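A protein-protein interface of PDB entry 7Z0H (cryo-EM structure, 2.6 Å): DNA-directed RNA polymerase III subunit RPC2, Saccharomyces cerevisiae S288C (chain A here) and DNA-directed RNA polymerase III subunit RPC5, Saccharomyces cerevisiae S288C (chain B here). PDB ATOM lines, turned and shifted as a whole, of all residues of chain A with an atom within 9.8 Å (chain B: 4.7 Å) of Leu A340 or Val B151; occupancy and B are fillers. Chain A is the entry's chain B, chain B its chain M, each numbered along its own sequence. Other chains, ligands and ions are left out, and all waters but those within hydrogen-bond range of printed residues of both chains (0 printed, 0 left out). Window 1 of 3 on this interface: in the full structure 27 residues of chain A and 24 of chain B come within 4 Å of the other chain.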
ATOM      1  N   ALA A 259     -25.582  10.482  13.165  1.00  0.00           N
ATOM      2  CA  ALA A 259     -25.472  11.909  12.901  1.00  0.00           C
ATOM      3  C   ALA A 259     -24.050  12.421  13.077  1.00  0.00           C
ATOM      4  O   ALA A 259     -23.698  13.454  12.499  1.00  0.00           O
ATOM      5  CB  ALA A 259     -26.421  12.683  13.815  1.00  0.00           C
ATOM      6  N   CYS A 260     -23.224  11.731  13.861  1.00  0.00           N
ATOM      7  CA  CYS A 260     -21.834  12.123  14.050  1.00  0.00           C
ATOM      8  C   CYS A 260     -20.898  11.410  13.080  1.00  0.00           C
ATOM      9  O   CYS A 260     -19.722  11.201  13.390  1.00  0.00           O
ATOM     10  CB  CYS A 260     -21.407  11.874  15.496  1.00  0.00           C
ATOM     11  SG  CYS A 260     -22.296  12.877  16.707  1.00  0.00           S
ATOM     12  N   GLY A 261     -21.403  11.021  11.912  1.00  0.00           N
ATOM     13  CA  GLY A 261     -20.586  10.440  10.871  1.00  0.00           C
ATOM     14  C   GLY A 261     -20.354   8.950  10.985  1.00  0.00           C
ATOM     15  O   GLY A 261     -19.906   8.335  10.011  1.00  0.00           O
ATOM     16  N   ILE A 262     -20.648   8.350  12.136  1.00  0.00           N
ATOM     17  CA  ILE A 262     -20.419   6.922  12.352  1.00  0.00           C
ATOM     18  C   ILE A 262     -21.722   6.233  11.957  1.00  0.00           C
ATOM     19  O   ILE A 262     -22.663   6.128  12.743  1.00  0.00           O
ATOM     20  CB  ILE A 262     -20.001   6.626  13.790  1.00  0.00           C
ATOM     21  CG1 ILE A 262     -18.575   7.136  14.023  1.00  0.00           C
ATOM     22  CG2 ILE A 262     -20.091   5.138  14.097  1.00  0.00           C
ATOM     23  CD1 ILE A 262     -17.488   6.153  13.708  1.00  0.00           C
ATOM     24  N   LEU A 263     -21.784   5.771  10.707  1.00  0.00           N
ATOM     25  CA  LEU A 263     -23.047   5.358  10.114  1.00  0.00           C
ATOM     26  C   LEU A 263     -23.035   3.978   9.470  1.00  0.00           C
ATOM     27  O   LEU A 263     -23.946   3.675   8.693  1.00  0.00           O
ATOM     28  CB  LEU A 263     -23.497   6.394   9.070  1.00  0.00           C
ATOM     29  CG  LEU A 263     -22.547   6.624   7.893  1.00  0.00           C
ATOM     30  CD1 LEU A 263     -23.102   5.999   6.626  1.00  0.00           C
ATOM     31  CD2 LEU A 263     -22.276   8.107   7.693  1.00  0.00           C
ATOM     32  N   GLN A 298     -26.410   9.525   6.949  1.00  0.00           N
ATOM     33  CA  GLN A 298     -25.983  10.496   7.950  1.00  0.00           C
ATOM     34  C   GLN A 298     -26.922  11.695   7.973  1.00  0.00           C
ATOM     35  O   GLN A 298     -27.392  12.108   9.039  1.00  0.00           O
ATOM     36  CB  GLN A 298     -24.546  10.944   7.678  1.00  0.00           C
ATOM     37  CG  GLN A 298     -24.188  12.278   8.320  1.00  0.00           C
ATOM     38  CD  GLN A 298     -22.697  12.551   8.324  1.00  0.00           C
ATOM     39  OE1 GLN A 298     -21.893  11.685   7.978  1.00  0.00           O
ATOM     40  NE2 GLN A 298     -22.318  13.761   8.720  1.00  0.00           N
ATOM     41  N   LEU A 302     -29.227  13.532  10.802  1.00  0.00           N
ATOM     42  CA  LEU A 302     -28.973  14.951  11.025  1.00  0.00           C
ATOM     43  C   LEU A 302     -30.278  15.735  11.073  1.00  0.00           C
ATOM     44  O   LEU A 302     -30.528  16.494  12.016  1.00  0.00           O
ATOM     45  CB  LEU A 302     -28.065  15.500   9.922  1.00  0.00           C
ATOM     46  CG  LEU A 302     -26.641  14.965   9.783  1.00  0.00           C
ATOM     47  CD1 LEU A 302     -25.861  15.741   8.732  1.00  0.00           C
ATOM     48  CD2 LEU A 302     -25.930  14.992  11.104  1.00  0.00           C
ATOM     49  N   GLU A 322     -31.774  21.479   7.759  1.00  0.00           N
ATOM     50  CA  GLU A 322     -30.774  20.509   8.188  1.00  0.00           C
ATOM     51  C   GLU A 322     -29.530  21.197   8.742  1.00  0.00           C
ATOM     52  O   GLU A 322     -28.748  20.565   9.456  1.00  0.00           O
ATOM     53  CB  GLU A 322     -30.420  19.585   7.016  1.00  0.00           C
ATOM     54  CG  GLU A 322     -29.353  18.540   7.306  1.00  0.00           C
ATOM     55  CD  GLU A 322     -27.994  18.938   6.775  1.00  0.00           C
ATOM     56  OE1 GLU A 322     -27.914  19.342   5.597  1.00  0.00           O
ATOM     57  OE2 GLU A 322     -27.006  18.853   7.535  1.00  0.00           O
ATOM     58  N   GLU A 325     -29.035  21.270  12.779  1.00  0.00           N
ATOM     59  CA  GLU A 325     -28.433  20.155  13.498  1.00  0.00           C
ATOM     60  C   GLU A 325     -26.931  20.326  13.625  1.00  0.00           C
ATOM     61  O   GLU A 325     -26.325  19.771  14.543  1.00  0.00           O
ATOM     62  CB  GLU A 325     -28.772  18.829  12.813  1.00  0.00           C
ATOM     63  CG  GLU A 325     -28.054  18.501  11.493  1.00  0.00           C
ATOM     64  CD  GLU A 325     -26.549  18.294  11.615  1.00  0.00           C
ATOM     65  OE1 GLU A 325     -25.802  18.831  10.770  1.00  0.00           O
ATOM     66  OE2 GLU A 325     -26.113  17.636  12.583  1.00  0.00           O
ATOM     67  N   ALA A 326     -26.306  21.050  12.694  1.00  0.00           N
ATOM     68  CA  ALA A 326     -24.868  21.259  12.786  1.00  0.00           C
ATOM     69  C   ALA A 326     -24.517  22.034  14.046  1.00  0.00           C
ATOM     70  O   ALA A 326     -23.600  21.653  14.780  1.00  0.00           O
ATOM     71  CB  ALA A 326     -24.359  21.982  11.541  1.00  0.00           C
ATOM     72  N   THR A 330     -22.497  20.645  17.246  1.00  0.00           N
ATOM     73  CA  THR A 330     -21.282  21.372  17.591  1.00  0.00           C
ATOM     74  C   THR A 330     -21.378  22.023  18.966  1.00  0.00           C
ATOM     75  O   THR A 330     -20.348  22.254  19.607  1.00  0.00           O
ATOM     76  CB  THR A 330     -20.995  22.414  16.502  1.00  0.00           C
ATOM     77  OG1 THR A 330     -20.757  21.743  15.259  1.00  0.00           O
ATOM     78  CG2 THR A 330     -19.769  23.253  16.837  1.00  0.00           C
ATOM     79  N   THR A 336     -15.939  21.146  20.293  1.00  0.00           N
ATOM     80  CA  THR A 336     -16.431  21.912  19.155  1.00  0.00           C
ATOM     81  C   THR A 336     -15.789  21.416  17.865  1.00  0.00           C
ATOM     82  O   THR A 336     -14.563  21.307  17.767  1.00  0.00           O
ATOM     83  CB  THR A 336     -16.141  23.399  19.352  1.00  0.00           C
ATOM     84  OG1 THR A 336     -14.743  23.585  19.605  1.00  0.00           O
ATOM     85  CG2 THR A 336     -16.939  23.946  20.525  1.00  0.00           C
ATOM     86  N   VAL A 337     -16.625  21.110  16.878  1.00  0.00           N
ATOM     87  CA  VAL A 337     -16.174  20.600  15.590  1.00  0.00           C
ATOM     88  C   VAL A 337     -16.236  21.745  14.592  1.00  0.00           C
ATOM     89  O   VAL A 337     -17.290  22.363  14.406  1.00  0.00           O
ATOM     90  CB  VAL A 337     -17.027  19.408  15.127  1.00  0.00           C
ATOM     91  CG1 VAL A 337     -16.861  19.184  13.633  1.00  0.00           C
ATOM     92  CG2 VAL A 337     -16.656  18.156  15.906  1.00  0.00           C
ATOM     93  N   GLU A 338     -15.105  22.034  13.951  1.00  0.00           N
ATOM     94  CA  GLU A 338     -14.989  23.164  13.038  1.00  0.00           C
ATOM     95  C   GLU A 338     -14.587  22.708  11.639  1.00  0.00           C
ATOM     96  O   GLU A 338     -13.812  23.381  10.957  1.00  0.00           O
ATOM     97  CB  GLU A 338     -13.992  24.187  13.581  1.00  0.00           C
ATOM     98  CG  GLU A 338     -14.483  24.920  14.819  1.00  0.00           C
ATOM     99  CD  GLU A 338     -15.438  26.049  14.491  1.00  0.00           C
ATOM    100  OE1 GLU A 338     -15.256  26.694  13.436  1.00  0.00           O
ATOM    101  OE2 GLU A 338     -16.373  26.289  15.283  1.00  0.00           O
ATOM    102  N   ALA A 339     -15.113  21.569  11.203  1.00  0.00           N
ATOM    103  CA  ALA A 339     -14.794  21.011   9.895  1.00  0.00           C
ATOM    104  C   ALA A 339     -15.880  19.998   9.536  1.00  0.00           C
ATOM    105  O   ALA A 339     -16.941  19.963  10.170  1.00  0.00           O
ATOM    106  CB  ALA A 339     -13.382  20.400   9.898  1.00  0.00           C
ATOM    107  N   LEU A 340     -15.620  19.186   8.515  1.00  0.00           N
ATOM    108  CA  LEU A 340     -16.558  18.165   8.073  1.00  0.00           C
ATOM    109  C   LEU A 340     -16.292  16.800   8.694  1.00  0.00           C
ATOM    110  O   LEU A 340     -16.961  15.828   8.329  1.00  0.00           O
ATOM    111  CB  LEU A 340     -16.529  18.048   6.545  1.00  0.00           C
ATOM    112  CG  LEU A 340     -17.889  17.938   5.856  1.00  0.00           C
ATOM    113  CD1 LEU A 340     -18.696  19.203   6.079  1.00  0.00           C
ATOM    114  CD2 LEU A 340     -17.718  17.672   4.371  1.00  0.00           C
ATOM    115  N   ASP A 341     -15.342  16.700   9.618  1.00  0.00           N
ATOM    116  CA  ASP A 341     -15.024  15.441  10.280  1.00  0.00           C
ATOM    117  C   ASP A 341     -15.623  15.429  11.682  1.00  0.00           C
ATOM    118  O   ASP A 341     -15.376  16.338  12.481  1.00  0.00           O
ATOM    119  CB  ASP A 341     -13.510  15.217  10.333  1.00  0.00           C
ATOM    120  CG  ASP A 341     -12.774  16.320  11.071  1.00  0.00           C
ATOM    121  OD1 ASP A 341     -13.287  17.458  11.113  1.00  0.00           O
ATOM    122  OD2 ASP A 341     -11.677  16.052  11.606  1.00  0.00           O
ATOM    123  N   PHE A 342     -16.424  14.401  11.969  1.00  0.00           N
ATOM    124  CA  PHE A 342     -17.110  14.273  13.250  1.00  0.00           C
ATOM    125  C   PHE A 342     -16.602  13.085  14.056  1.00  0.00           C
ATOM    126  O   PHE A 342     -17.283  12.643  14.985  1.00  0.00           O
ATOM    127  CB  PHE A 342     -18.623  14.144  13.057  1.00  0.00           C
ATOM    128  CG  PHE A 342     -19.270  15.328  12.396  1.00  0.00           C
ATOM    129  CD1 PHE A 342     -19.025  15.629  11.066  1.00  0.00           C
ATOM    130  CD2 PHE A 342     -20.164  16.115  13.100  1.00  0.00           C
ATOM    131  CE1 PHE A 342     -19.635  16.709  10.466  1.00  0.00           C
ATOM    132  CE2 PHE A 342     -20.775  17.195  12.504  1.00  0.00           C
ATOM    133  CZ  PHE A 342     -20.512  17.492  11.188  1.00  0.00           C
ATOM    134  N   ARG A 343     -15.427  12.552  13.717  1.00  0.00           N
ATOM    135  CA  ARG A 343     -14.955  11.343  14.383  1.00  0.00           C
ATOM    136  C   ARG A 343     -14.696  11.575  15.866  1.00  0.00           C
ATOM    137  O   ARG A 343     -14.936  10.677  16.677  1.00  0.00           O
ATOM    138  CB  ARG A 343     -13.693  10.817  13.700  1.00  0.00           C
ATOM    139  CG  ARG A 343     -13.258   9.438  14.178  1.00  0.00           C
ATOM    140  CD  ARG A 343     -12.628   8.633  13.053  1.00  0.00           C
ATOM    141  NE  ARG A 343     -12.169   7.320  13.496  1.00  0.00           N
ATOM    142  CZ  ARG A 343     -12.950   6.256  13.622  1.00  0.00           C
ATOM    143  NH1 ARG A 343     -14.245   6.314  13.367  1.00  0.00           N
ATOM    144  NH2 ARG A 343     -12.416   5.101  14.010  1.00  0.00           N
ATOM    145  N   GLU A 344     -14.227  12.764  16.244  1.00  0.00           N
ATOM    146  CA  GLU A 344     -13.905  13.027  17.644  1.00  0.00           C
ATOM    147  C   GLU A 344     -15.159  13.000  18.515  1.00  0.00           C
ATOM    148  O   GLU A 344     -15.228  12.266  19.509  1.00  0.00           O
ATOM    149  CB  GLU A 344     -13.185  14.371  17.760  1.00  0.00           C
ATOM    150  CG  GLU A 344     -12.953  14.841  19.179  1.00  0.00           C
ATOM    151  CD  GLU A 344     -11.506  14.689  19.597  1.00  0.00           C
ATOM    152  OE1 GLU A 344     -10.864  13.710  19.162  1.00  0.00           O
ATOM    153  OE2 GLU A 344     -11.007  15.553  20.348  1.00  0.00           O
ATOM    154  N   ALA A 346     -18.004  11.747  17.626  1.00  0.00           N
ATOM    155  CA  ALA A 346     -18.610  10.435  17.455  1.00  0.00           C
ATOM    156  C   ALA A 346     -18.018   9.430  18.428  1.00  0.00           C
ATOM    157  O   ALA A 346     -18.747   8.677  19.080  1.00  0.00           O
ATOM    158  CB  ALA A 346     -18.424   9.964  16.015  1.00  0.00           C
ATOM    159  N   THR A 542      -8.299   9.085  13.872  1.00  0.00           N
ATOM    160  CA  THR A 542      -8.582   9.144  12.445  1.00  0.00           C
ATOM    161  C   THR A 542      -7.787   8.116  11.642  1.00  0.00           C
ATOM    162  O   THR A 542      -8.067   7.932  10.453  1.00  0.00           O
ATOM    163  CB  THR A 542      -8.314  10.556  11.918  1.00  0.00           C
ATOM    164  OG1 THR A 542      -6.921  10.860  12.043  1.00  0.00           O
ATOM    165  CG2 THR A 542      -9.123  11.583  12.696  1.00  0.00           C
ATOM    166  N   LEU A 543      -6.807   7.445  12.251  1.00  0.00           N
ATOM    167  CA  LEU A 543      -6.107   6.327  11.620  1.00  0.00           C
ATOM    168  C   LEU A 543      -6.574   4.967  12.113  1.00  0.00           C
ATOM    169  O   LEU A 543      -6.082   3.946  11.623  1.00  0.00           O
ATOM    170  CB  LEU A 543      -4.595   6.417  11.853  1.00  0.00           C
ATOM    171  CG  LEU A 543      -3.730   7.357  11.025  1.00  0.00           C
ATOM    172  CD1 LEU A 543      -4.055   7.194   9.545  1.00  0.00           C
ATOM    173  CD2 LEU A 543      -3.941   8.764  11.491  1.00  0.00           C
ATOM    174  N   SER B 116     -12.198  21.031   0.044  1.00  0.00           N
ATOM    175  CA  SER B 116     -12.967  20.392   1.107  1.00  0.00           C
ATOM    176  C   SER B 116     -12.570  18.947   1.366  1.00  0.00           C
ATOM    177  O   SER B 116     -12.943  18.409   2.414  1.00  0.00           O
ATOM    178  CB  SER B 116     -14.466  20.451   0.793  1.00  0.00           C
ATOM    179  OG  SER B 116     -15.235  20.067   1.917  1.00  0.00           O
ATOM    180  N   HIS B 117     -11.841  18.299   0.452  1.00  0.00           N
ATOM    181  CA  HIS B 117     -11.220  16.993   0.686  1.00  0.00           C
ATOM    182  C   HIS B 117     -12.260  15.901   0.950  1.00  0.00           C
ATOM    183  O   HIS B 117     -12.207  15.202   1.960  1.00  0.00           O
ATOM    184  CB  HIS B 117     -10.208  17.082   1.829  1.00  0.00           C
ATOM    185  CG  HIS B 117      -9.264  18.237   1.703  1.00  0.00           C
ATOM    186  ND1 HIS B 117      -8.376  18.361   0.657  1.00  0.00           N
ATOM    187  CD2 HIS B 117      -9.087  19.333   2.479  1.00  0.00           C
ATOM    188  CE1 HIS B 117      -7.682  19.477   0.801  1.00  0.00           C
ATOM    189  NE2 HIS B 117      -8.096  20.085   1.897  1.00  0.00           N
ATOM    190  N   LEU B 118     -13.201  15.748   0.023  1.00  0.00           N
ATOM    191  CA  LEU B 118     -14.174  14.664   0.073  1.00  0.00           C
ATOM    192  C   LEU B 118     -13.844  13.630  -0.994  1.00  0.00           C
ATOM    193  O   LEU B 118     -13.670  13.976  -2.165  1.00  0.00           O
ATOM    194  CB  LEU B 118     -15.600  15.178  -0.125  1.00  0.00           C
ATOM    195  CG  LEU B 118     -16.261  15.874   1.064  1.00  0.00           C
ATOM    196  CD1 LEU B 118     -16.320  17.363   0.824  1.00  0.00           C
ATOM    197  CD2 LEU B 118     -17.652  15.310   1.315  1.00  0.00           C
ATOM    198  N   LYS B 149     -18.142   7.330   0.774  1.00  0.00           N
ATOM    199  CA  LYS B 149     -17.715   8.708   0.975  1.00  0.00           C
ATOM    200  C   LYS B 149     -16.956   8.825   2.289  1.00  0.00           C
ATOM    201  O   LYS B 149     -17.388   8.286   3.314  1.00  0.00           O
ATOM    202  CB  LYS B 149     -18.908   9.665   0.972  1.00  0.00           C
ATOM    203  CG  LYS B 149     -18.508  11.134   0.980  1.00  0.00           C
ATOM    204  CD  LYS B 149     -19.706  12.040   1.191  1.00  0.00           C
ATOM    205  CE  LYS B 149     -19.844  12.438   2.653  1.00  0.00           C
ATOM    206  NZ  LYS B 149     -20.719  13.630   2.827  1.00  0.00           N
ATOM    207  N   GLY B 150     -15.826   9.526   2.252  1.00  0.00           N
ATOM    208  CA  GLY B 150     -15.056   9.788   3.450  1.00  0.00           C
ATOM    209  C   GLY B 150     -14.111  10.957   3.279  1.00  0.00           C
ATOM    210  O   GLY B 150     -13.351  11.011   2.309  1.00  0.00           O
ATOM    211  N   VAL B 151     -14.146  11.898   4.217  1.00  0.00           N
ATOM    212  CA  VAL B 151     -13.297  13.081   4.147  1.00  0.00           C
ATOM    213  C   VAL B 151     -11.878  12.689   4.535  1.00  0.00           C
ATOM    214  O   VAL B 151     -11.645  12.178   5.635  1.00  0.00           O
ATOM    215  CB  VAL B 151     -13.828  14.200   5.053  1.00  0.00           C
ATOM    216  CG1 VAL B 151     -12.845  15.359   5.098  1.00  0.00           C
ATOM    217  CG2 VAL B 151     -15.188  14.673   4.568  1.00  0.00           C
ATOM    218  N   GLY B 152     -10.932  12.914   3.627  1.00  0.00           N
ATOM    219  CA  GLY B 152      -9.533  12.721   3.947  1.00  0.00           C
ATOM    220  C   GLY B 152      -9.094  13.668   5.044  1.00  0.00           C
ATOM    221  O   GLY B 152      -9.310  14.879   4.944  1.00  0.00           O
ATOM    222  N   VAL B 153      -8.482  13.134   6.097  1.00  0.00           N
ATOM    223  CA  VAL B 153      -8.127  13.906   7.281  1.00  0.00           C
ATOM    224  C   VAL B 153      -6.623  14.130   7.287  1.00  0.00           C
ATOM    225  O   VAL B 153      -5.843  13.179   7.152  1.00  0.00           O
ATOM    226  CB  VAL B 153      -8.594  13.209   8.572  1.00  0.00           C
ATOM    227  CG1 VAL B 153     -10.080  13.446   8.790  1.00  0.00           C
ATOM    228  CG2 VAL B 153      -8.302  11.723   8.508  1.00  0.00           C
ATOM    229  N   VAL B 176      -5.060  10.892   4.902  1.00  0.00           N
ATOM    230  CA  VAL B 176      -5.672   9.571   4.998  1.00  0.00           C
ATOM    231  C   VAL B 176      -7.188   9.706   4.999  1.00  0.00           C
ATOM    232  O   VAL B 176      -7.751  10.621   5.613  1.00  0.00           O
ATOM    233  CB  VAL B 176      -5.184   8.847   6.264  1.00  0.00           C
ATOM    234  CG1 VAL B 176      -5.504   7.364   6.188  1.00  0.00           C
ATOM    235  CG2 VAL B 176      -3.696   9.070   6.463  1.00  0.00           C
ATOM    236  N   ALA B 177      -7.859   8.794   4.300  1.00  0.00           N
ATOM    237  CA  ALA B 177      -9.304   8.847   4.119  1.00  0.00           C
ATOM    238  C   ALA B 177      -9.951   7.586   4.673  1.00  0.00           C
ATOM    239  O   ALA B 177      -9.502   6.473   4.391  1.00  0.00           O
ATOM    240  CB  ALA B 177      -9.666   9.009   2.639  1.00  0.00           C
ATOM    241  N   GLN B 178     -11.016   7.769   5.450  1.00  0.00           N
ATOM    242  CA  GLN B 178     -11.773   6.670   6.043  1.00  0.00           C
ATOM    243  C   GLN B 178     -13.101   6.562   5.299  1.00  0.00           C
ATOM    244  O   GLN B 178     -14.036   7.323   5.563  1.00  0.00           O
ATOM    245  CB  GLN B 178     -11.980   6.895   7.537  1.00  0.00           C
ATOM    246  CG  GLN B 178     -10.790   6.484   8.387  1.00  0.00           C
ATOM    247  CD  GLN B 178     -11.198   5.770   9.657  1.00  0.00           C
ATOM    248  OE1 GLN B 178     -10.500   4.875  10.130  1.00  0.00           O
ATOM    249  NE2 GLN B 178     -12.333   6.168  10.222  1.00  0.00           N
ATOM    250  N   ALA B 233     -18.585  24.708   6.758  1.00  0.00           N
ATOM    251  CA  ALA B 233     -17.988  23.513   6.170  1.00  0.00           C
ATOM    252  C   ALA B 233     -18.984  22.787   5.274  1.00  0.00           C
ATOM    253  O   ALA B 233     -18.701  22.525   4.100  1.00  0.00           O
ATOM    254  CB  ALA B 233     -17.478  22.586   7.274  1.00  0.00           C
ATOM    255  N   HIS B 234     -20.171  22.479   5.803  1.00  0.00           N
ATOM    256  CA  HIS B 234     -21.177  21.792   4.999  1.00  0.00           C
ATOM    257  C   HIS B 234     -21.712  22.691   3.892  1.00  0.00           C
ATOM    258  O   HIS B 234     -22.005  22.216   2.787  1.00  0.00           O
ATOM    259  CB  HIS B 234     -22.317  21.295   5.886  1.00  0.00           C
ATOM    260  CG  HIS B 234     -21.887  20.303   6.919  1.00  0.00           C
ATOM    261  ND1 HIS B 234     -22.114  18.949   6.789  1.00  0.00           N
ATOM    262  CD2 HIS B 234     -21.244  20.465   8.099  1.00  0.00           C
ATOM    263  CE1 HIS B 234     -21.628  18.321   7.845  1.00  0.00           C
ATOM    264  NE2 HIS B 234     -21.096  19.217   8.655  1.00  0.00           N
ATOM    265  N   ALA B 237     -19.193  22.526   1.242  1.00  0.00           N
ATOM    266  CA  ALA B 237     -19.112  21.177   0.692  1.00  0.00           C
ATOM    267  C   ALA B 237     -20.245  20.897  -0.285  1.00  0.00           C
ATOM    268  O   ALA B 237     -20.022  20.308  -1.349  1.00  0.00           O
ATOM    269  CB  ALA B 237     -19.116  20.151   1.825  1.00  0.00           C
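NE2 of Gln B178 sits close to NE of Arg A343.
The backbone NH of Val B153 is in hydrogen-bond range of the backbone carbonyl oxygen of Val B176.
Among the printed residues, pairs that only touch across the chains: Phe A342 with His B234 (3.1 Å), Leu A340 with His B234 (3.5 Å), Thr A542 with Val B153 (3.6 Å), Leu A543 with Val B176 (3.6 Å), Leu A340 with Ala B233 (3.7 Å), Thr A542 with Gln B178 (3.7 Å), Ala A339 with Ala B233 (3.8 Å), Leu A340 with Ala B237 (3.8 Å), Leu A340 with Leu B118 (3.8 Å) and Leu A340 with Val B151 (3.9 Å).
Of chain B, only Leu B118 (3.8 Å), Val B151 (3.9 Å), Ala B233 (3.7 Å), His B234 (3.5 Å) and Ala B237 (3.8 Å) come within 4 Å of Leu A340.
Val B151 touches one residue of chain A.
No residue of chain A comes within 4 Å of Gly B152.
Of the printed residues of chain A, His B234 touches Leu A340 and Phe A342.
Printed residues of chain A within 4 Å of Leu B118: Leu A340 (3.8 Å).
Printed residues of chain A within 4 Å of Val B153: Thr A542 (3.6 Å).
Printed residues of chain B within 4 Å of Arg A343: Gln B178.
Thr A330 touches none of the printed residues of chain B.
Leu A302 touches none of the printed residues of chain B.
The nearest printed residue of chain B that does not touch Leu A543 is Gln B178 (4.4 Å).
Of the 14 printed residues of chain B, 8 touch a printed residue of chain A.
Of the 23 printed residues of chain A, 6 touch a printed residue of chain B.
Hydrophobic or aromatic side chains of chain A that line the printed part of chain B: Leu A340, Phe A342 and Leu A543.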
